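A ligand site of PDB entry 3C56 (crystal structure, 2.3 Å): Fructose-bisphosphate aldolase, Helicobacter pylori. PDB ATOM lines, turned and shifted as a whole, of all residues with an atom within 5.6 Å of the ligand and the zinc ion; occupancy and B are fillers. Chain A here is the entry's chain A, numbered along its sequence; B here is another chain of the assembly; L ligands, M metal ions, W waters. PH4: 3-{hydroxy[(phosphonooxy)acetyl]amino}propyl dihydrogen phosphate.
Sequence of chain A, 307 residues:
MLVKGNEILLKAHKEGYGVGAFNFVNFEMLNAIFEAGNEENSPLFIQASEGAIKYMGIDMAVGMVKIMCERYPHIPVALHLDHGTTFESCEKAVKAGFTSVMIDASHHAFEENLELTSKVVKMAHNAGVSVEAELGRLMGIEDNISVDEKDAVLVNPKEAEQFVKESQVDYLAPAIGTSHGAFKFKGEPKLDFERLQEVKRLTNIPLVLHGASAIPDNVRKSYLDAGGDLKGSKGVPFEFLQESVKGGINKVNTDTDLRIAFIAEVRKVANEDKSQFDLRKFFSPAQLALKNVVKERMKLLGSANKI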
ATOM      1  N   ASN A  23      -5.145 -24.851 -33.934  1.00  0.00           N
ATOM      2  CA  ASN A  23      -5.521 -23.668 -34.690  1.00  0.00           C
ATOM      3  C   ASN A  23      -4.387 -23.176 -35.569  1.00  0.00           C
ATOM      4  O   ASN A  23      -3.212 -23.396 -35.281  1.00  0.00           O
ATOM      5  CB  ASN A  23      -5.980 -22.550 -33.751  1.00  0.00           C
ATOM      6  CG  ASN A  23      -7.217 -22.917 -32.961  1.00  0.00           C
ATOM      7  OD1 ASN A  23      -7.175 -23.805 -32.108  1.00  0.00           O
ATOM      8  ND2 ASN A  23      -8.325 -22.231 -33.236  1.00  0.00           N
ATOM      9  N   GLN A  47      -8.372 -26.488 -37.093  1.00  0.00           N
ATOM     10  CA  GLN A  47      -9.476 -25.555 -36.912  1.00  0.00           C
ATOM     11  C   GLN A  47      -9.068 -24.099 -37.066  1.00  0.00           C
ATOM     12  O   GLN A  47      -7.909 -23.739 -36.862  1.00  0.00           O
ATOM     13  CB  GLN A  47     -10.138 -25.786 -35.542  1.00  0.00           C
ATOM     14  CG  GLN A  47      -9.180 -25.731 -34.366  1.00  0.00           C
ATOM     15  CD  GLN A  47      -9.850 -26.112 -33.060  1.00  0.00           C
ATOM     16  OE1 GLN A  47     -10.782 -26.909 -33.047  1.00  0.00           O
ATOM     17  NE2 GLN A  47      -9.372 -25.545 -31.967  1.00  0.00           N
ATOM     18  N   SER A  49     -10.570 -20.075 -36.118  1.00  0.00           N
ATOM     19  CA  SER A  49     -11.541 -19.186 -35.504  1.00  0.00           C
ATOM     20  C   SER A  49     -12.108 -18.238 -36.554  1.00  0.00           C
ATOM     21  O   SER A  49     -11.592 -18.149 -37.672  1.00  0.00           O
ATOM     22  CB  SER A  49     -10.886 -18.381 -34.381  1.00  0.00           C
ATOM     23  OG  SER A  49      -9.816 -17.601 -34.880  1.00  0.00           O
ATOM     24  N   GLY A  51     -11.902 -15.153 -36.328  1.00  0.00           N
ATOM     25  CA  GLY A  51     -10.868 -14.141 -36.462  1.00  0.00           C
ATOM     26  C   GLY A  51      -9.791 -14.573 -37.433  1.00  0.00           C
ATOM     27  O   GLY A  51      -9.238 -13.744 -38.167  1.00  0.00           O
ATOM     28  N   ALA A  52      -9.492 -15.862 -37.433  1.00  0.00           N
ATOM     29  CA  ALA A  52      -8.497 -16.418 -38.353  1.00  0.00           C
ATOM     30  C   ALA A  52      -9.032 -16.395 -39.784  1.00  0.00           C
ATOM     31  O   ALA A  52      -8.300 -16.082 -40.718  1.00  0.00           O
ATOM     32  CB  ALA A  52      -8.142 -17.835 -37.945  1.00  0.00           C
ATOM     33  N   ASP A  82     -13.781 -22.986 -35.665  1.00  0.00           N
ATOM     34  CA  ASP A  82     -13.644 -22.821 -34.229  1.00  0.00           C
ATOM     35  C   ASP A  82     -14.433 -21.621 -33.713  1.00  0.00           C
ATOM     36  O   ASP A  82     -14.182 -20.478 -34.100  1.00  0.00           O
ATOM     37  CB  ASP A  82     -12.169 -22.695 -33.847  1.00  0.00           C
ATOM     38  CG  ASP A  82     -11.954 -22.762 -32.352  1.00  0.00           C
ATOM     39  OD1 ASP A  82     -12.856 -23.247 -31.628  1.00  0.00           O
ATOM     40  OD2 ASP A  82     -10.874 -22.326 -31.898  1.00  0.00           O
ATOM     41  N   HIS A  83     -15.400 -21.897 -32.832  1.00  0.00           N
ATOM     42  CA  HIS A  83     -16.199 -20.851 -32.209  1.00  0.00           C
ATOM     43  C   HIS A  83     -17.014 -20.033 -33.213  1.00  0.00           C
ATOM     44  O   HIS A  83     -16.904 -18.809 -33.262  1.00  0.00           O
ATOM     45  CB  HIS A  83     -15.336 -19.923 -31.353  1.00  0.00           C
ATOM     46  CG  HIS A  83     -14.950 -20.508 -30.028  1.00  0.00           C
ATOM     47  ND1 HIS A  83     -15.805 -20.531 -28.949  1.00  0.00           N
ATOM     48  CD2 HIS A  83     -13.802 -21.085 -29.612  1.00  0.00           C
ATOM     49  CE1 HIS A  83     -15.199 -21.099 -27.919  1.00  0.00           C
ATOM     50  NE2 HIS A  83     -13.979 -21.439 -28.301  1.00  0.00           N
ATOM     51  N   LEU A 138     -16.889 -20.766 -20.447  1.00  0.00           N
ATOM     52  CA  LEU A 138     -15.448 -21.011 -20.358  1.00  0.00           C
ATOM     53  C   LEU A 138     -14.775 -20.032 -19.414  1.00  0.00           C
ATOM     54  O   LEU A 138     -14.188 -19.043 -19.863  1.00  0.00           O
ATOM     55  CB  LEU A 138     -14.799 -20.902 -21.746  1.00  0.00           C
ATOM     56  CG  LEU A 138     -14.941 -22.116 -22.646  1.00  0.00           C
ATOM     57  CD1 LEU A 138     -14.231 -21.883 -23.974  1.00  0.00           C
ATOM     58  CD2 LEU A 138     -14.429 -23.357 -21.929  1.00  0.00           C
ATOM     59  N   SER A 179      -9.935 -22.404 -19.687  1.00  0.00           N
ATOM     60  CA  SER A 179     -10.176 -21.110 -20.319  1.00  0.00           C
ATOM     61  C   SER A 179      -9.070 -20.813 -21.318  1.00  0.00           C
ATOM     62  O   SER A 179      -7.982 -21.392 -21.237  1.00  0.00           O
ATOM     63  CB  SER A 179     -10.256 -20.005 -19.265  1.00  0.00           C
ATOM     64  OG  SER A 179      -9.019 -19.837 -18.604  1.00  0.00           O
ATOM     65  N   HIS A 180      -9.328 -19.917 -22.261  1.00  0.00           N
ATOM     66  CA  HIS A 180      -8.347 -19.562 -23.270  1.00  0.00           C
ATOM     67  C   HIS A 180      -7.297 -18.605 -22.713  1.00  0.00           C
ATOM     68  O   HIS A 180      -7.543 -17.896 -21.732  1.00  0.00           O
ATOM     69  CB  HIS A 180      -9.023 -18.921 -24.492  1.00  0.00           C
ATOM     70  CG  HIS A 180     -10.230 -19.684 -24.976  1.00  0.00           C
ATOM     71  ND1 HIS A 180     -11.420 -19.059 -25.277  1.00  0.00           N
ATOM     72  CD2 HIS A 180     -10.421 -21.001 -25.201  1.00  0.00           C
ATOM     73  CE1 HIS A 180     -12.299 -19.972 -25.673  1.00  0.00           C
ATOM     74  NE2 HIS A 180     -11.719 -21.156 -25.624  1.00  0.00           N
ATOM     75  N   GLY A 181      -6.130 -18.584 -23.337  1.00  0.00           N
ATOM     76  CA  GLY A 181      -5.048 -17.697 -22.922  1.00  0.00           C
ATOM     77  C   GLY A 181      -3.967 -18.421 -22.150  1.00  0.00           C
ATOM     78  O   GLY A 181      -4.092 -19.609 -21.834  1.00  0.00           O
ATOM     79  N   ALA A 182      -2.888 -17.712 -21.846  1.00  0.00           N
ATOM     80  CA  ALA A 182      -1.773 -18.293 -21.109  1.00  0.00           C
ATOM     81  C   ALA A 182      -1.996 -18.236 -19.603  1.00  0.00           C
ATOM     82  O   ALA A 182      -1.235 -18.815 -18.828  1.00  0.00           O
ATOM     83  CB  ALA A 182      -0.468 -17.615 -21.488  1.00  0.00           C
ATOM     84  N   LYS A 184      -4.575 -19.348 -17.179  1.00  0.00           N
ATOM     85  CA  LYS A 184      -5.764 -20.127 -16.876  1.00  0.00           C
ATOM     86  C   LYS A 184      -5.963 -20.299 -15.374  1.00  0.00           C
ATOM     87  O   LYS A 184      -7.079 -20.190 -14.873  1.00  0.00           O
ATOM     88  CB  LYS A 184      -5.675 -21.503 -17.528  1.00  0.00           C
ATOM     89  CG  LYS A 184      -5.280 -21.472 -18.997  1.00  0.00           C
ATOM     90  CD  LYS A 184      -5.121 -22.872 -19.554  1.00  0.00           C
ATOM     91  CE  LYS A 184      -4.592 -22.838 -20.968  1.00  0.00           C
ATOM     92  NZ  LYS A 184      -5.412 -21.971 -21.846  1.00  0.00           N
ATOM     93  N   LEU A 209     -12.405 -30.402 -25.156  1.00  0.00           N
ATOM     94  CA  LEU A 209     -11.848 -29.564 -24.100  1.00  0.00           C
ATOM     95  C   LEU A 209     -11.247 -28.289 -24.690  1.00  0.00           C
ATOM     96  O   LEU A 209     -10.300 -28.347 -25.485  1.00  0.00           O
ATOM     97  CB  LEU A 209     -10.781 -30.319 -23.305  1.00  0.00           C
ATOM     98  CG  LEU A 209     -10.309 -29.644 -22.013  1.00  0.00           C
ATOM     99  CD1 LEU A 209     -11.404 -29.692 -20.960  1.00  0.00           C
ATOM    100  CD2 LEU A 209      -9.038 -30.304 -21.483  1.00  0.00           C
ATOM    101  N   HIS A 210     -11.794 -27.146 -24.301  1.00  0.00           N
ATOM    102  CA  HIS A 210     -11.304 -25.861 -24.775  1.00  0.00           C
ATOM    103  C   HIS A 210     -10.232 -25.317 -23.840  1.00  0.00           C
ATOM    104  O   HIS A 210     -10.108 -25.764 -22.700  1.00  0.00           O
ATOM    105  CB  HIS A 210     -12.450 -24.849 -24.896  1.00  0.00           C
ATOM    106  CG  HIS A 210     -13.268 -25.024 -26.145  1.00  0.00           C
ATOM    107  ND1 HIS A 210     -13.326 -24.066 -27.127  1.00  0.00           N
ATOM    108  CD2 HIS A 210     -14.064 -26.041 -26.556  1.00  0.00           C
ATOM    109  CE1 HIS A 210     -14.123 -24.483 -28.096  1.00  0.00           C
ATOM    110  NE2 HIS A 210     -14.587 -25.673 -27.772  1.00  0.00           N
ATOM    111  N   GLY A 211      -9.455 -24.358 -24.319  1.00  0.00           N
ATOM    112  CA  GLY A 211      -8.388 -23.763 -23.530  1.00  0.00           C
ATOM    113  C   GLY A 211      -7.539 -24.823 -22.861  1.00  0.00           C
ATOM    114  O   GLY A 211      -7.375 -24.815 -21.638  1.00  0.00           O
ATOM    115  N   ALA A 212      -7.003 -25.746 -23.657  1.00  0.00           N
ATOM    116  CA  ALA A 212      -6.285 -26.889 -23.114  1.00  0.00           C
ATOM    117  C   ALA A 212      -4.779 -26.826 -23.359  1.00  0.00           C
ATOM    118  O   ALA A 212      -4.103 -27.853 -23.374  1.00  0.00           O
ATOM    119  CB  ALA A 212      -6.861 -28.179 -23.679  1.00  0.00           C
ATOM    120  N   SER A 213      -4.261 -25.620 -23.572  1.00  0.00           N
ATOM    121  CA  SER A 213      -2.825 -25.432 -23.712  1.00  0.00           C
ATOM    122  C   SER A 213      -2.129 -25.674 -22.372  1.00  0.00           C
ATOM    123  O   SER A 213      -2.674 -25.338 -21.321  1.00  0.00           O
ATOM    124  CB  SER A 213      -2.507 -24.025 -24.216  1.00  0.00           C
ATOM    125  OG  SER A 213      -2.598 -23.958 -25.626  1.00  0.00           O
ATOM    126  N   ASN A 253      -8.448 -28.726 -27.814  1.00  0.00           N
ATOM    127  CA  ASN A 253      -8.111 -27.458 -28.453  1.00  0.00           C
ATOM    128  C   ASN A 253      -6.760 -26.905 -27.991  1.00  0.00           C
ATOM    129  O   ASN A 253      -6.556 -26.640 -26.805  1.00  0.00           O
ATOM    130  CB  ASN A 253      -9.217 -26.431 -28.211  1.00  0.00           C
ATOM    131  CG  ASN A 253     -10.503 -26.780 -28.955  1.00  0.00           C
ATOM    132  OD1 ASN A 253     -10.710 -27.924 -29.351  1.00  0.00           O
ATOM    133  ND2 ASN A 253     -11.369 -25.789 -29.134  1.00  0.00           N
ATOM    134  N   THR A 254      -5.852 -26.740 -28.943  1.00  0.00           N
ATOM    135  CA  THR A 254      -4.527 -26.193 -28.663  1.00  0.00           C
ATOM    136  C   THR A 254      -4.215 -25.030 -29.583  1.00  0.00           C
ATOM    137  O   THR A 254      -4.304 -25.146 -30.812  1.00  0.00           O
ATOM    138  CB  THR A 254      -3.426 -27.261 -28.819  1.00  0.00           C
ATOM    139  OG1 THR A 254      -3.862 -28.494 -28.228  1.00  0.00           O
ATOM    140  CG2 THR A 254      -2.146 -26.805 -28.158  1.00  0.00           C
ATOM    141  N   ASP A 255      -3.838 -23.890 -28.999  1.00  0.00           N
ATOM    142  CA  ASP A 255      -3.576 -22.679 -29.766  1.00  0.00           C
ATOM    143  C   ASP A 255      -2.464 -21.842 -29.142  1.00  0.00           C
ATOM    144  O   ASP A 255      -1.486 -21.517 -29.807  1.00  0.00           O
ATOM    145  CB  ASP A 255      -4.854 -21.847 -29.892  1.00  0.00           C
ATOM    146  CG  ASP A 255      -4.729 -20.716 -30.906  1.00  0.00           C
ATOM    147  OD1 ASP A 255      -3.605 -20.243 -31.139  1.00  0.00           O
ATOM    148  OD2 ASP A 255      -5.769 -20.303 -31.462  1.00  0.00           O
ATOM    149  N   THR A 256      -2.620 -21.510 -27.865  1.00  0.00           N
ATOM    150  CA  THR A 256      -1.655 -20.668 -27.167  1.00  0.00           C
ATOM    151  C   THR A 256      -0.244 -21.247 -27.225  1.00  0.00           C
ATOM    152  O   THR A 256       0.718 -20.525 -27.500  1.00  0.00           O
ATOM    153  CB  THR A 256      -2.050 -20.453 -25.695  1.00  0.00           C
ATOM    154  OG1 THR A 256      -3.295 -19.744 -25.636  1.00  0.00           O
ATOM    155  CG2 THR A 256      -0.982 -19.634 -24.981  1.00  0.00           C
ATOM    156  N   ASP A 257      -0.118 -22.535 -26.959  1.00  0.00           N
ATOM    157  CA  ASP A 257       1.176 -23.209 -27.011  1.00  0.00           C
ATOM    158  C   ASP A 257       1.871 -22.987 -28.349  1.00  0.00           C
ATOM    159  O   ASP A 257       3.075 -22.742 -28.403  1.00  0.00           O
ATOM    160  CB  ASP A 257       1.012 -24.712 -26.743  1.00  0.00           C
ATOM    161  CG  ASP A 257       0.713 -25.022 -25.290  1.00  0.00           C
ATOM    162  OD1 ASP A 257       0.936 -24.138 -24.442  1.00  0.00           O
ATOM    163  OD2 ASP A 257       0.243 -26.135 -25.005  1.00  0.00           O
ATOM    164  N   ARG A 259       1.277 -20.491 -30.624  1.00  0.00           N
ATOM    165  CA  ARG A 259       1.632 -19.079 -30.745  1.00  0.00           C
ATOM    166  C   ARG A 259       2.942 -18.767 -30.027  1.00  0.00           C
ATOM    167  O   ARG A 259       3.885 -18.246 -30.614  1.00  0.00           O
ATOM    168  CB  ARG A 259       0.522 -18.186 -30.188  1.00  0.00           C
ATOM    169  CG  ARG A 259      -0.832 -18.328 -30.875  1.00  0.00           C
ATOM    170  CD  ARG A 259      -1.808 -17.263 -30.382  1.00  0.00           C
ATOM    171  NE  ARG A 259      -3.169 -17.505 -30.847  1.00  0.00           N
ATOM    172  CZ  ARG A 259      -4.193 -16.700 -30.579  1.00  0.00           C
ATOM    173  NH1 ARG A 259      -4.012 -15.603 -29.846  1.00  0.00           N
ATOM    174  NH2 ARG A 259      -5.398 -16.990 -31.033  1.00  0.00           N
ATOM    175  N   ASP B 278       0.378 -13.118 -30.472  1.00  0.00           N
ATOM    176  CA  ASP B 278      -0.647 -13.332 -31.482  1.00  0.00           C
ATOM    177  C   ASP B 278      -0.082 -12.960 -32.851  1.00  0.00           C
ATOM    178  O   ASP B 278       0.120 -11.777 -33.143  1.00  0.00           O
ATOM    179  CB  ASP B 278      -1.892 -12.504 -31.174  1.00  0.00           C
ATOM    180  CG  ASP B 278      -3.027 -12.767 -32.152  1.00  0.00           C
ATOM    181  OD1 ASP B 278      -2.803 -13.446 -33.168  1.00  0.00           O
ATOM    182  OD2 ASP B 278      -4.157 -12.283 -31.893  1.00  0.00           O
ATOM    183  N   ARG B 280      -1.209 -12.626 -35.746  1.00  0.00           N
ATOM    184  CA  ARG B 280      -1.988 -11.653 -36.514  1.00  0.00           C
ATOM    185  C   ARG B 280      -1.680 -10.214 -36.086  1.00  0.00           C
ATOM    186  O   ARG B 280      -1.846  -9.282 -36.877  1.00  0.00           O
ATOM    187  CB  ARG B 280      -3.479 -11.955 -36.384  1.00  0.00           C
ATOM    188  CG  ARG B 280      -3.910 -13.233 -37.075  1.00  0.00           C
ATOM    189  CD  ARG B 280      -5.296 -13.667 -36.645  1.00  0.00           C
ATOM    190  NE  ARG B 280      -5.361 -13.913 -35.212  1.00  0.00           N
ATOM    191  CZ  ARG B 280      -6.395 -14.494 -34.602  1.00  0.00           C
ATOM    192  NH1 ARG B 280      -7.451 -14.873 -35.303  1.00  0.00           N
ATOM    193  NH2 ARG B 280      -6.379 -14.688 -33.292  1.00  0.00           N
HETATM  194  N3  PH4 L   1      -9.609 -22.270 -29.111  1.00  0.00           N
HETATM  195  C4  PH4 L   1      -8.952 -21.245 -29.923  1.00  0.00           C
HETATM  196  C5  PH4 L   1      -9.935 -20.071 -30.147  1.00  0.00           C
HETATM  197  C6  PH4 L   1      -9.307 -19.048 -31.111  1.00  0.00           C
HETATM  198  O62 PH4 L   1      -8.282 -16.957 -32.862  1.00  0.00           O
HETATM  199  P6  PH4 L   1      -8.960 -16.445 -31.452  1.00  0.00           P
HETATM  200  O63 PH4 L   1      -7.871 -15.546 -30.615  1.00  0.00           O
HETATM  201  O61 PH4 L   1     -10.143 -15.653 -31.742  1.00  0.00           O
HETATM  202  O6  PH4 L   1      -9.393 -17.769 -30.549  1.00  0.00           O
HETATM  203  O3  PH4 L   1     -10.796 -22.866 -29.552  1.00  0.00           O
HETATM  204  C2  PH4 L   1      -9.003 -22.684 -27.846  1.00  0.00           C
HETATM  205  O2  PH4 L   1      -9.531 -23.517 -27.181  1.00  0.00           O
HETATM  206  C1  PH4 L   1      -7.694 -22.034 -27.357  1.00  0.00           C
HETATM  207  O1  PH4 L   1      -7.216 -22.728 -26.237  1.00  0.00           O
HETATM  208  P1  PH4 L   1      -5.786 -22.274 -25.551  1.00  0.00           P
HETATM  209  O12 PH4 L   1      -5.737 -20.635 -25.395  1.00  0.00           O
HETATM  210  O13 PH4 L   1      -4.541 -22.771 -26.509  1.00  0.00           O
HETATM  211  O11 PH4 L   1      -5.658 -22.892 -24.231  1.00  0.00           O
HETATM  212 ZN    ZN M   1     -12.124 -22.294 -27.508  1.00  0.00          ZN
HETATM  213  O   HOH W   1     -12.194 -15.734 -33.266  1.00  0.00           O
HETATM  214  O   HOH W   2     -12.472 -18.007 -31.549  1.00  0.00           O
HETATM  215  O   HOH W   3      -9.564 -13.421 -33.041  1.00  0.00           O
HETATM  216  O   HOH W   4      -6.245 -19.107 -27.744  1.00  0.00           O
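The side-chain amino group (NZ) of Lys 184 is in salt-bridge range of an oxygen (O11) of the ligand (2.6 Å). The backbone NH of Ala 212 sits at hydrogen-bond distance from an oxygen (O11) of the ligand, at 3.2 Å. N of Gly 211 is in hydrogen-bond range of O2 of the ligand, 3.0 Å away. An oxygen (O11) of the ligand lies within hydrogen-bond range of the backbone NH of Ser 213 (3.1 Å). The backbone NH (N) of Asp 255 sits at hydrogen-bond distance from an oxygen (O13) of the ligand (2.8 Å). An oxygen (O12) of the ligand sits at hydrogen-bond distance from the backbone NH (N) of Gly 181, 2.9 Å away. The guanidinium group (NH2) of Arg 280 of chain B is in salt-bridge range of an oxygen (O62) of the ligand. The backbone NH (N) of Thr 256 sits at hydrogen-bond distance from an oxygen (O13) of the ligand, 2.7 Å away. ND2 of Asn 253 sits close to O3 of the ligand (3.0 Å). An oxygen (O62) of the ligand sits at hydrogen-bond distance from the side-chain hydroxyl of Ser 49 (2.6 Å). The side-chain carboxylate of Asp 82 sits close to an oxygen (O3) of the ligand. The guanidinium group (NH2) of Arg 259 is in salt-bridge range of an oxygen (O63) of the ligand (2.9 Å). The side-chain hydroxyl (OG) of Ser 213 sits at hydrogen-bond distance from an oxygen (O13) of the ligand. An oxygen (O12) of the ligand is in hydrogen-bond range of the side-chain hydroxyl (OG1) of Thr 256 (2.6 Å).
The side-chain amide oxygen (OD1) of Asn 23 sits at hydrogen-bond distance from the side-chain amide nitrogen (NE2) of Gln 47, at 2.8 Å. OD2 of Asp 82 sits at hydrogen-bond distance from ND2 of Asn 23, 2.9 Å away. The backbone carbonyl oxygen (O) of Ser 179 lies within hydrogen-bond range of the side-chain amino group (NZ) of Lys 184. The side-chain hydroxyl of Ser 213 sits at hydrogen-bond distance from the backbone NH of Thr 256 (3.3 Å). OG of Ser 213 sits at hydrogen-bond distance from N of Asp 257 (3.2 Å). O of Gly 211 is in hydrogen-bond range of NZ of Lys 184 (3.5 Å). The backbone NH of Ala 52 is in hydrogen-bond range of the side-chain hydroxyl of Ser 49. The side-chain carboxylate of Asp 255 lies within salt-bridge range of the guanidinium group of Arg 259 (2.8 Å).
Merely in contact with the ligand: Asn 23 (3.5 Å), Thr 254 (3.8 Å) and Gln 47 (3.9 Å). 18 residues have an atom within 4 Å of the ligand: Asn 23, Gln 47, Ser 49, Asp 82, His 83, His 180, Gly 181, Lys 184, His 210, Gly 211, Ala 212, Ser 213, Asn 253, Thr 254, Asp 255, Thr 256, Arg 259 and Arg 280 of chain B. The nearest printed residue that does not touch the ligand is Ser 179 (4.1 Å).
Residues that only touch the zinc ion: Asn 253 (3.9 Å). Of the 26 residues printed, 4 come within 4 Å of the zinc ion.
The zinc ion is bound by ND1 of His 210, NE2 of His 83, NE2 of His 180 and O3 of the ligand.
Water W1 lies within hydrogen-bond range of O61 of the ligand (2.6 Å), N of Gly 51 (3.1 Å) and OG of Ser 49 (3.4 Å). Water W3 lies within hydrogen-bond range of O61 of the ligand (2.6 Å) and NH1 of Arg 280 of chain B (3.4 Å).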
